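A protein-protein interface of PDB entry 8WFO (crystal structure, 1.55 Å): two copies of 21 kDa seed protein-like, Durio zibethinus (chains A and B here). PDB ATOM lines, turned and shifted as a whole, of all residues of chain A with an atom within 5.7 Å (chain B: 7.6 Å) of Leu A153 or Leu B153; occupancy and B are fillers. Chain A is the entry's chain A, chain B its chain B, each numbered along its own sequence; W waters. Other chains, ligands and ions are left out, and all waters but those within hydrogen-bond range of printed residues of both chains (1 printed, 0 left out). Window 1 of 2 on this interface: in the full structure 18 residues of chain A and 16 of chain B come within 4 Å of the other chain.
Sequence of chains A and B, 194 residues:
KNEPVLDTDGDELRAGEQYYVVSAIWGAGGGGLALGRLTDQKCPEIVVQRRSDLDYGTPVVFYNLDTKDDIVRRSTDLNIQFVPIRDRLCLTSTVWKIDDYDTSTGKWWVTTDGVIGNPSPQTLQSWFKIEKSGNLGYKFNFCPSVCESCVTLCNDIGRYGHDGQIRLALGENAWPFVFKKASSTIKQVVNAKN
Of chain B, only Leu B153 (3.8 Å) comes within 4 Å of Leu A153. Leu B153 touches just these residues of chain A: Thr A152 (3.9 Å) and Leu A153 (3.8 Å). Printed residues of chain A within 4 Å of Asn B155: Val A151 (3.8 Å). Printed residues of chain A within 4 Å of Leu B170: Val A151 (3.9 Å). The nearest printed residue of chain B that does not touch Leu A153 is Val B151 (4.1 Å).
Along chain B the printed residues that touch a printed residue of chain A span positions 108 to 170. Among the printed residues, 9 pairs touch across the chains.
Trp A108 touches Trp B108 (CH2 to CH2, 3.7 Å). Val A151 touches Asn B155 (CG2 to OD1, 3.8 Å). Val A151 touches Leu B170. CD2 of Leu B153 touches C of Thr A152 (3.9 Å). CD2 of Leu B153 touches N of Leu A153 (3.8 Å). OD1 of Asn A155 touches CG1 of Val B151 (3.2 Å). CG2 of Val B151 touches O of Leu A170, 3.9 Å away.
The backbone carbonyl oxygen (O) of Trp A108 is in hydrogen-bond range of the backbone NH (N) of Leu A170 (3.0 Å). N of Phe A142 lies within hydrogen-bond range of O of Asn A155 (2.8 Å). O of Trp B108 sits at hydrogen-bond distance from N of Leu B170, at 3.0 Å. The backbone carbonyl oxygen (O) of Asn B155 lies close to the side-chain amide oxygen (OD1) of Asn B141, 3.4 Å away. N of Asn B155 is in hydrogen-bond range of O of Phe B142 (2.8 Å). The side-chain sulfur of Cys B143 is disulfide-bonded to the side-chain sulfur of Cys B154 (2.0 Å).
Trp B108 touches its own counterpart, Trp A108. Trp A108 touches Val B151, and with the chains exchanged Val A151 touches Trp B108. Val A151 touches Asn B155, and with the chains exchanged Asn A155 touches Val B151. Leu A153 touches its own counterpart, Leu B153. Of the 9 pairs that touch across the chains among the printed residues, 8 have their exchanged pair printed and touching as well.
Water W1 lies within hydrogen-bond range of OD1 of Asn A155 (2.8 Å), O of Thr B152 (3.0 Å) and N of Cys A154 (3.3 Å).
The indole nitrogen of Trp A108 sits at hydrogen-bond distance from the backbone carbonyl oxygen of Val B151. The backbone carbonyl oxygen of Val A151 lies within hydrogen-bond range of the indole nitrogen of Trp B108.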
ATOM      1  N   ILE A  98      -8.088   1.171   7.271  1.00  0.00           N
ATOM      2  CA  ILE A  98      -8.903   0.778   8.417  1.00  0.00           C
ATOM      3  C   ILE A  98     -10.371   0.842   8.010  1.00  0.00           C
ATOM      4  O   ILE A  98     -10.816   1.826   7.417  1.00  0.00           O
ATOM      5  CB  ILE A  98      -8.621   1.672   9.632  1.00  0.00           C
ATOM      6  CG1 ILE A  98      -7.157   1.532  10.033  1.00  0.00           C
ATOM      7  CG2 ILE A  98      -9.522   1.285  10.787  1.00  0.00           C
ATOM      8  CD1 ILE A  98      -6.784   0.102  10.432  1.00  0.00           C
ATOM      9  N   TRP A 108     -12.132  -3.152  14.501  1.00  0.00           N
ATOM     10  CA  TRP A 108     -11.732  -2.263  13.418  1.00  0.00           C
ATOM     11  C   TRP A 108     -10.755  -3.049  12.544  1.00  0.00           C
ATOM     12  O   TRP A 108      -9.554  -3.115  12.841  1.00  0.00           O
ATOM     13  CB  TRP A 108     -11.062  -1.008  13.965  1.00  0.00           C
ATOM     14  CG  TRP A 108     -11.874  -0.166  14.905  1.00  0.00           C
ATOM     15  CD1 TRP A 108     -11.941  -0.287  16.258  1.00  0.00           C
ATOM     16  CD2 TRP A 108     -12.692   0.948  14.555  1.00  0.00           C
ATOM     17  NE1 TRP A 108     -12.766   0.696  16.787  1.00  0.00           N
ATOM     18  CE2 TRP A 108     -13.232   1.466  15.755  1.00  0.00           C
ATOM     19  CE3 TRP A 108     -13.017   1.568  13.346  1.00  0.00           C
ATOM     20  CZ2 TRP A 108     -14.077   2.569  15.773  1.00  0.00           C
ATOM     21  CZ3 TRP A 108     -13.865   2.659  13.366  1.00  0.00           C
ATOM     22  CH2 TRP A 108     -14.373   3.157  14.575  1.00  0.00           C
ATOM     23  N   PHE A 142      -1.701   2.067  13.656  1.00  0.00           N
ATOM     24  CA  PHE A 142      -2.552   3.035  12.991  1.00  0.00           C
ATOM     25  C   PHE A 142      -2.715   4.222  13.925  1.00  0.00           C
ATOM     26  O   PHE A 142      -3.376   4.108  14.957  1.00  0.00           O
ATOM     27  CB  PHE A 142      -3.910   2.447  12.644  1.00  0.00           C
ATOM     28  CG  PHE A 142      -4.803   3.425  11.975  1.00  0.00           C
ATOM     29  CD1 PHE A 142      -4.575   3.802  10.675  1.00  0.00           C
ATOM     30  CD2 PHE A 142      -5.838   4.024  12.671  1.00  0.00           C
ATOM     31  CE1 PHE A 142      -5.373   4.722  10.043  1.00  0.00           C
ATOM     32  CE2 PHE A 142      -6.642   4.953  12.058  1.00  0.00           C
ATOM     33  CZ  PHE A 142      -6.424   5.312  10.744  1.00  0.00           C
ATOM     34  N   CYS A 143      -2.120   5.341  13.562  1.00  0.00           N
ATOM     35  CA  CYS A 143      -2.202   6.547  14.376  1.00  0.00           C
ATOM     36  C   CYS A 143      -1.770   7.735  13.528  1.00  0.00           C
ATOM     37  O   CYS A 143      -0.719   8.338  13.785  1.00  0.00           O
ATOM     38  CB  CYS A 143      -1.337   6.389  15.618  1.00  0.00           C
ATOM     39  SG  CYS A 143      -1.607   7.674  16.824  1.00  0.00           S
ATOM     40  N   PRO A 144      -2.524   8.069  12.485  1.00  0.00           N
ATOM     41  CA  PRO A 144      -2.013   9.016  11.488  1.00  0.00           C
ATOM     42  C   PRO A 144      -1.816  10.413  12.055  1.00  0.00           C
ATOM     43  O   PRO A 144      -2.582  10.877  12.906  1.00  0.00           O
ATOM     44  CB  PRO A 144      -3.084   8.994  10.392  1.00  0.00           C
ATOM     45  CG  PRO A 144      -4.289   8.436  11.041  1.00  0.00           C
ATOM     46  CD  PRO A 144      -3.809   7.475  12.071  1.00  0.00           C
ATOM     47  N   VAL A 151      -9.695  13.967  14.625  1.00  0.00           N
ATOM     48  CA  VAL A 151      -9.758  12.941  15.651  1.00  0.00           C
ATOM     49  C   VAL A 151      -9.554  11.589  14.988  1.00  0.00           C
ATOM     50  O   VAL A 151     -10.184  11.291  13.966  1.00  0.00           O
ATOM     51  CB  VAL A 151     -11.118  13.000  16.369  1.00  0.00           C
ATOM     52  CG1 VAL A 151     -11.288  11.820  17.314  1.00  0.00           C
ATOM     53  CG2 VAL A 151     -11.297  14.331  17.069  1.00  0.00           C
ATOM     54  N   THR A 152      -8.699  10.759  15.579  1.00  0.00           N
ATOM     55  CA  THR A 152      -8.313   9.491  14.971  1.00  0.00           C
ATOM     56  C   THR A 152      -8.181   8.400  16.024  1.00  0.00           C
ATOM     57  O   THR A 152      -7.875   8.660  17.191  1.00  0.00           O
ATOM     58  CB  THR A 152      -6.984   9.613  14.206  1.00  0.00           C
ATOM     59  OG1 THR A 152      -6.689   8.357  13.590  1.00  0.00           O
ATOM     60  CG2 THR A 152      -5.832   9.986  15.145  1.00  0.00           C
ATOM     61  N   LEU A 153      -8.423   7.166  15.588  1.00  0.00           N
ATOM     62  CA  LEU A 153      -7.958   6.004  16.321  1.00  0.00           C
ATOM     63  C   LEU A 153      -6.435   6.036  16.398  1.00  0.00           C
ATOM     64  O   LEU A 153      -5.760   6.666  15.582  1.00  0.00           O
ATOM     65  CB  LEU A 153      -8.419   4.720  15.620  1.00  0.00           C
ATOM     66  CG  LEU A 153      -9.955   4.561  15.559  1.00  0.00           C
ATOM     67  CD1 LEU A 153     -10.378   3.721  14.348  1.00  0.00           C
ATOM     68  CD2 LEU A 153     -10.461   3.937  16.844  1.00  0.00           C
ATOM     69  N   CYS A 154      -5.899   5.382  17.420  1.00  0.00           N
ATOM     70  CA  CYS A 154      -4.451   5.409  17.626  1.00  0.00           C
ATOM     71  C   CYS A 154      -4.090   4.105  18.340  1.00  0.00           C
ATOM     72  O   CYS A 154      -4.106   4.027  19.570  1.00  0.00           O
ATOM     73  CB  CYS A 154      -4.027   6.638  18.411  1.00  0.00           C
ATOM     74  SG  CYS A 154      -2.250   6.774  18.552  1.00  0.00           S
ATOM     75  N   ASN A 155      -3.810   3.068  17.555  1.00  0.00           N
ATOM     76  CA  ASN A 155      -3.662   1.740  18.126  1.00  0.00           C
ATOM     77  C   ASN A 155      -2.771   0.858  17.274  1.00  0.00           C
ATOM     78  O   ASN A 155      -2.717   0.987  16.046  1.00  0.00           O
ATOM     79  CB  ASN A 155      -4.991   0.988  18.308  1.00  0.00           C
ATOM     80  CG  ASN A 155      -6.001   1.763  19.112  1.00  0.00           C
ATOM     81  OD1 ASN A 155      -6.694   2.652  18.608  1.00  0.00           O
ATOM     82  ND2 ASN A 155      -6.054   1.454  20.400  1.00  0.00           N
ATOM     83  N   LEU A 170      -7.224  -3.513  14.647  1.00  0.00           N
ATOM     84  CA  LEU A 170      -6.660  -2.769  15.761  1.00  0.00           C
ATOM     85  C   LEU A 170      -6.829  -3.574  17.045  1.00  0.00           C
ATOM     86  O   LEU A 170      -7.834  -4.267  17.238  1.00  0.00           O
ATOM     87  CB  LEU A 170      -7.349  -1.408  15.897  1.00  0.00           C
ATOM     88  CG  LEU A 170      -7.326  -0.506  14.661  1.00  0.00           C
ATOM     89  CD1 LEU A 170      -8.059   0.816  14.968  1.00  0.00           C
ATOM     90  CD2 LEU A 170      -5.913  -0.255  14.194  1.00  0.00           C
ATOM     91  N   ILE B  98     -22.407   7.604  17.482  1.00  0.00           N
ATOM     92  CA  ILE B  98     -21.297   8.112  16.685  1.00  0.00           C
ATOM     93  C   ILE B  98     -21.356   7.450  15.317  1.00  0.00           C
ATOM     94  O   ILE B  98     -21.501   6.226  15.209  1.00  0.00           O
ATOM     95  CB  ILE B  98     -19.947   7.866  17.372  1.00  0.00           C
ATOM     96  CG1 ILE B  98     -19.888   8.646  18.670  1.00  0.00           C
ATOM     97  CG2 ILE B  98     -18.801   8.297  16.454  1.00  0.00           C
ATOM     98  CD1 ILE B  98     -20.132  10.131  18.469  1.00  0.00           C
ATOM     99  N   ASP B  99     -21.272   8.264  14.274  1.00  0.00           N
ATOM    100  CA  ASP B  99     -21.310   7.806  12.890  1.00  0.00           C
ATOM    101  C   ASP B  99     -19.982   7.160  12.478  1.00  0.00           C
ATOM    102  O   ASP B  99     -18.968   7.224  13.182  1.00  0.00           O
ATOM    103  CB  ASP B  99     -21.627   8.987  11.969  1.00  0.00           C
ATOM    104  CG  ASP B  99     -22.290   8.580  10.667  1.00  0.00           C
ATOM    105  OD1 ASP B  99     -22.529   7.372  10.420  1.00  0.00           O
ATOM    106  OD2 ASP B  99     -22.564   9.501   9.862  1.00  0.00           O
ATOM    107  N   ASP B 100     -20.004   6.529  11.312  1.00  0.00           N
ATOM    108  CA  ASP B 100     -18.760   6.120  10.674  1.00  0.00           C
ATOM    109  C   ASP B 100     -18.004   7.359  10.218  1.00  0.00           C
ATOM    110  O   ASP B 100     -18.596   8.395   9.924  1.00  0.00           O
ATOM    111  CB  ASP B 100     -19.044   5.213   9.475  1.00  0.00           C
ATOM    112  CG  ASP B 100     -19.751   3.950   9.871  1.00  0.00           C
ATOM    113  OD1 ASP B 100     -19.254   3.235  10.765  1.00  0.00           O
ATOM    114  OD2 ASP B 100     -20.842   3.693   9.312  1.00  0.00           O
ATOM    115  N   TYR B 101     -16.678   7.250  10.158  1.00  0.00           N
ATOM    116  CA  TYR B 101     -15.860   8.384   9.748  1.00  0.00           C
ATOM    117  C   TYR B 101     -16.304   8.936   8.395  1.00  0.00           C
ATOM    118  O   TYR B 101     -16.532   8.182   7.444  1.00  0.00           O
ATOM    119  CB  TYR B 101     -14.400   7.939   9.677  1.00  0.00           C
ATOM    120  CG  TYR B 101     -13.446   9.034   9.270  1.00  0.00           C
ATOM    121  CD1 TYR B 101     -13.176  10.095  10.124  1.00  0.00           C
ATOM    122  CD2 TYR B 101     -12.799   8.994   8.041  1.00  0.00           C
ATOM    123  CE1 TYR B 101     -12.291  11.101   9.763  1.00  0.00           C
ATOM    124  CE2 TYR B 101     -11.911   9.996   7.668  1.00  0.00           C
ATOM    125  CZ  TYR B 101     -11.658  11.037   8.530  1.00  0.00           C
ATOM    126  OH  TYR B 101     -10.780  12.035   8.174  1.00  0.00           O
ATOM    127  N   TRP B 108     -16.085  12.722  12.782  1.00  0.00           N
ATOM    128  CA  TRP B 108     -16.915  11.669  13.364  1.00  0.00           C
ATOM    129  C   TRP B 108     -18.157  12.360  13.919  1.00  0.00           C
ATOM    130  O   TRP B 108     -18.137  12.897  15.031  1.00  0.00           O
ATOM    131  CB  TRP B 108     -16.182  10.930  14.476  1.00  0.00           C
ATOM    132  CG  TRP B 108     -14.890  10.275  14.080  1.00  0.00           C
ATOM    133  CD1 TRP B 108     -13.649  10.843  14.080  1.00  0.00           C
ATOM    134  CD2 TRP B 108     -14.707   8.902  13.722  1.00  0.00           C
ATOM    135  NE1 TRP B 108     -12.700   9.912  13.697  1.00  0.00           N
ATOM    136  CE2 TRP B 108     -13.327   8.714  13.481  1.00  0.00           C
ATOM    137  CE3 TRP B 108     -15.579   7.821  13.553  1.00  0.00           C
ATOM    138  CZ2 TRP B 108     -12.799   7.486  13.101  1.00  0.00           C
ATOM    139  CZ3 TRP B 108     -15.051   6.596  13.174  1.00  0.00           C
ATOM    140  CH2 TRP B 108     -13.672   6.442  12.949  1.00  0.00           C
ATOM    141  N   LEU B 124     -21.650  -0.294  20.955  1.00  0.00           N
ATOM    142  CA  LEU B 124     -20.580   0.575  21.451  1.00  0.00           C
ATOM    143  C   LEU B 124     -20.754   2.030  21.020  1.00  0.00           C
ATOM    144  O   LEU B 124     -20.449   2.955  21.788  1.00  0.00           O
ATOM    145  CB  LEU B 124     -19.228   0.040  20.977  1.00  0.00           C
ATOM    146  CG  LEU B 124     -17.988   0.513  21.730  1.00  0.00           C
ATOM    147  CD1 LEU B 124     -18.092   0.182  23.192  1.00  0.00           C
ATOM    148  CD2 LEU B 124     -16.774  -0.168  21.129  1.00  0.00           C
ATOM    149  N   GLN B 125     -21.242   2.255  19.802  1.00  0.00           N
ATOM    150  CA  GLN B 125     -21.355   3.610  19.281  1.00  0.00           C
ATOM    151  C   GLN B 125     -22.477   4.416  19.929  1.00  0.00           C
ATOM    152  O   GLN B 125     -22.564   5.619  19.666  1.00  0.00           O
ATOM    153  CB  GLN B 125     -21.579   3.571  17.767  1.00  0.00           C
ATOM    154  CG  GLN B 125     -20.446   2.925  16.995  1.00  0.00           C
ATOM    155  CD  GLN B 125     -20.882   2.350  15.674  1.00  0.00           C
ATOM    156  OE1 GLN B 125     -21.781   1.507  15.614  1.00  0.00           O
ATOM    157  NE2 GLN B 125     -20.204   2.768  14.591  1.00  0.00           N
ATOM    158  N   ASN B 141     -18.860  13.430  26.138  1.00  0.00           N
ATOM    159  CA  ASN B 141     -17.597  12.740  25.937  1.00  0.00           C
ATOM    160  C   ASN B 141     -17.918  11.366  25.373  1.00  0.00           C
ATOM    161  O   ASN B 141     -18.723  10.630  25.954  1.00  0.00           O
ATOM    162  CB  ASN B 141     -16.861  12.665  27.280  1.00  0.00           C
ATOM    163  CG  ASN B 141     -15.629  11.813  27.233  1.00  0.00           C
ATOM    164  OD1 ASN B 141     -15.002  11.678  26.191  1.00  0.00           O
ATOM    165  ND2 ASN B 141     -15.231  11.282  28.388  1.00  0.00           N
ATOM    166  N   PHE B 142     -17.349  11.028  24.216  1.00  0.00           N
ATOM    167  CA  PHE B 142     -17.519   9.683  23.684  1.00  0.00           C
ATOM    168  C   PHE B 142     -16.275   8.893  24.047  1.00  0.00           C
ATOM    169  O   PHE B 142     -15.221   9.073  23.440  1.00  0.00           O
ATOM    170  CB  PHE B 142     -17.738   9.670  22.176  1.00  0.00           C
ATOM    171  CG  PHE B 142     -17.931   8.281  21.622  1.00  0.00           C
ATOM    172  CD1 PHE B 142     -19.096   7.582  21.895  1.00  0.00           C
ATOM    173  CD2 PHE B 142     -16.930   7.652  20.891  1.00  0.00           C
ATOM    174  CE1 PHE B 142     -19.299   6.303  21.426  1.00  0.00           C
ATOM    175  CE2 PHE B 142     -17.102   6.368  20.425  1.00  0.00           C
ATOM    176  CZ  PHE B 142     -18.287   5.677  20.676  1.00  0.00           C
ATOM    177  N   CYS B 143     -16.404   8.027  25.031  1.00  0.00           N
ATOM    178  CA  CYS B 143     -15.255   7.220  25.437  1.00  0.00           C
ATOM    179  C   CYS B 143     -15.777   5.964  26.122  1.00  0.00           C
ATOM    180  O   CYS B 143     -15.599   5.801  27.337  1.00  0.00           O
ATOM    181  CB  CYS B 143     -14.348   8.027  26.363  1.00  0.00           C
ATOM    182  SG  CYS B 143     -12.811   7.145  26.683  1.00  0.00           S
ATOM    183  N   PRO B 144     -16.490   5.099  25.401  1.00  0.00           N
ATOM    184  CA  PRO B 144     -17.220   4.021  26.074  1.00  0.00           C
ATOM    185  C   PRO B 144     -16.283   3.018  26.722  1.00  0.00           C
ATOM    186  O   PRO B 144     -15.214   2.691  26.192  1.00  0.00           O
ATOM    187  CB  PRO B 144     -18.048   3.386  24.951  1.00  0.00           C
ATOM    188  CG  PRO B 144     -17.361   3.785  23.686  1.00  0.00           C
ATOM    189  CD  PRO B 144     -16.758   5.131  23.951  1.00  0.00           C
ATOM    190  N   SER B 145     -16.695   2.537  27.893  1.00  0.00           N
ATOM    191  CA  SER B 145     -15.943   1.516  28.610  1.00  0.00           C
ATOM    192  C   SER B 145     -16.781   0.271  28.861  1.00  0.00           C
ATOM    193  O   SER B 145     -16.409  -0.566  29.688  1.00  0.00           O
ATOM    194  CB  SER B 145     -15.396   2.080  29.923  1.00  0.00           C
ATOM    195  OG  SER B 145     -16.390   2.771  30.654  1.00  0.00           O
ATOM    196  N   CYS B 150     -12.504  -3.833  23.541  1.00  0.00           N
ATOM    197  CA  CYS B 150     -12.777  -3.140  22.292  1.00  0.00           C
ATOM    198  C   CYS B 150     -11.895  -1.912  22.206  1.00  0.00           C
ATOM    199  O   CYS B 150     -11.798  -1.139  23.167  1.00  0.00           O
ATOM    200  CB  CYS B 150     -14.245  -2.719  22.175  1.00  0.00           C
ATOM    201  SG  CYS B 150     -15.427  -4.068  21.965  1.00  0.00           S
ATOM    202  N   VAL B 151     -11.259  -1.733  21.053  1.00  0.00           N
ATOM    203  CA  VAL B 151     -10.623  -0.469  20.732  1.00  0.00           C
ATOM    204  C   VAL B 151     -11.706   0.551  20.422  1.00  0.00           C
ATOM    205  O   VAL B 151     -12.656   0.265  19.678  1.00  0.00           O
ATOM    206  CB  VAL B 151      -9.674  -0.639  19.538  1.00  0.00           C
ATOM    207  CG1 VAL B 151      -9.225   0.720  19.012  1.00  0.00           C
ATOM    208  CG2 VAL B 151      -8.473  -1.509  19.927  1.00  0.00           C
ATOM    209  N   THR B 152     -11.570   1.747  20.984  1.00  0.00           N
ATOM    210  CA  THR B 152     -12.595   2.763  20.821  1.00  0.00           C
ATOM    211  C   THR B 152     -11.963   4.130  20.632  1.00  0.00           C
ATOM    212  O   THR B 152     -10.848   4.394  21.093  1.00  0.00           O
ATOM    213  CB  THR B 152     -13.548   2.800  22.029  1.00  0.00           C
ATOM    214  OG1 THR B 152     -14.542   3.811  21.819  1.00  0.00           O
ATOM    215  CG2 THR B 152     -12.786   3.104  23.318  1.00  0.00           C
ATOM    216  N   LEU B 153     -12.701   5.008  19.951  1.00  0.00           N
ATOM    217  CA  LEU B 153     -12.431   6.434  20.064  1.00  0.00           C
ATOM    218  C   LEU B 153     -12.680   6.891  21.496  1.00  0.00           C
ATOM    219  O   LEU B 153     -13.453   6.283  22.239  1.00  0.00           O
ATOM    220  CB  LEU B 153     -13.317   7.223  19.099  1.00  0.00           C
ATOM    221  CG  LEU B 153     -13.053   6.892  17.629  1.00  0.00           C
ATOM    222  CD1 LEU B 153     -14.302   7.197  16.807  1.00  0.00           C
ATOM    223  CD2 LEU B 153     -11.833   7.665  17.126  1.00  0.00           C
ATOM    224  N   CYS B 154     -11.984   7.951  21.896  1.00  0.00           N
ATOM    225  CA  CYS B 154     -12.118   8.479  23.253  1.00  0.00           C
ATOM    226  C   CYS B 154     -11.884   9.987  23.148  1.00  0.00           C
ATOM    227  O   CYS B 154     -10.745  10.452  23.182  1.00  0.00           O
ATOM    228  CB  CYS B 154     -11.135   7.806  24.205  1.00  0.00           C
ATOM    229  SG  CYS B 154     -11.292   8.282  25.916  1.00  0.00           S
ATOM    230  N   ASN B 155     -12.975  10.742  22.999  1.00  0.00           N
ATOM    231  CA  ASN B 155     -12.816  12.151  22.672  1.00  0.00           C
ATOM    232  C   ASN B 155     -14.077  12.921  23.032  1.00  0.00           C
ATOM    233  O   ASN B 155     -15.190  12.401  22.923  1.00  0.00           O
ATOM    234  CB  ASN B 155     -12.505  12.307  21.182  1.00  0.00           C
ATOM    235  CG  ASN B 155     -11.686  13.535  20.874  1.00  0.00           C
ATOM    236  OD1 ASN B 155     -10.468  13.442  20.694  1.00  0.00           O
ATOM    237  ND2 ASN B 155     -12.346  14.682  20.749  1.00  0.00           N
ATOM    238  N   LEU B 170     -16.980  14.610  17.242  1.00  0.00           N
ATOM    239  CA  LEU B 170     -15.816  14.531  18.107  1.00  0.00           C
ATOM    240  C   LEU B 170     -14.869  15.653  17.706  1.00  0.00           C
ATOM    241  O   LEU B 170     -14.754  15.979  16.521  1.00  0.00           O
ATOM    242  CB  LEU B 170     -15.132  13.166  17.961  1.00  0.00           C
ATOM    243  CG  LEU B 170     -16.025  11.942  18.208  1.00  0.00           C
ATOM    244  CD1 LEU B 170     -15.208  10.638  18.083  1.00  0.00           C
ATOM    245  CD2 LEU B 170     -16.703  12.029  19.560  1.00  0.00           C
HETATM  246  O   HOH W   1      -8.244   4.673  19.649  1.00  0.00           O
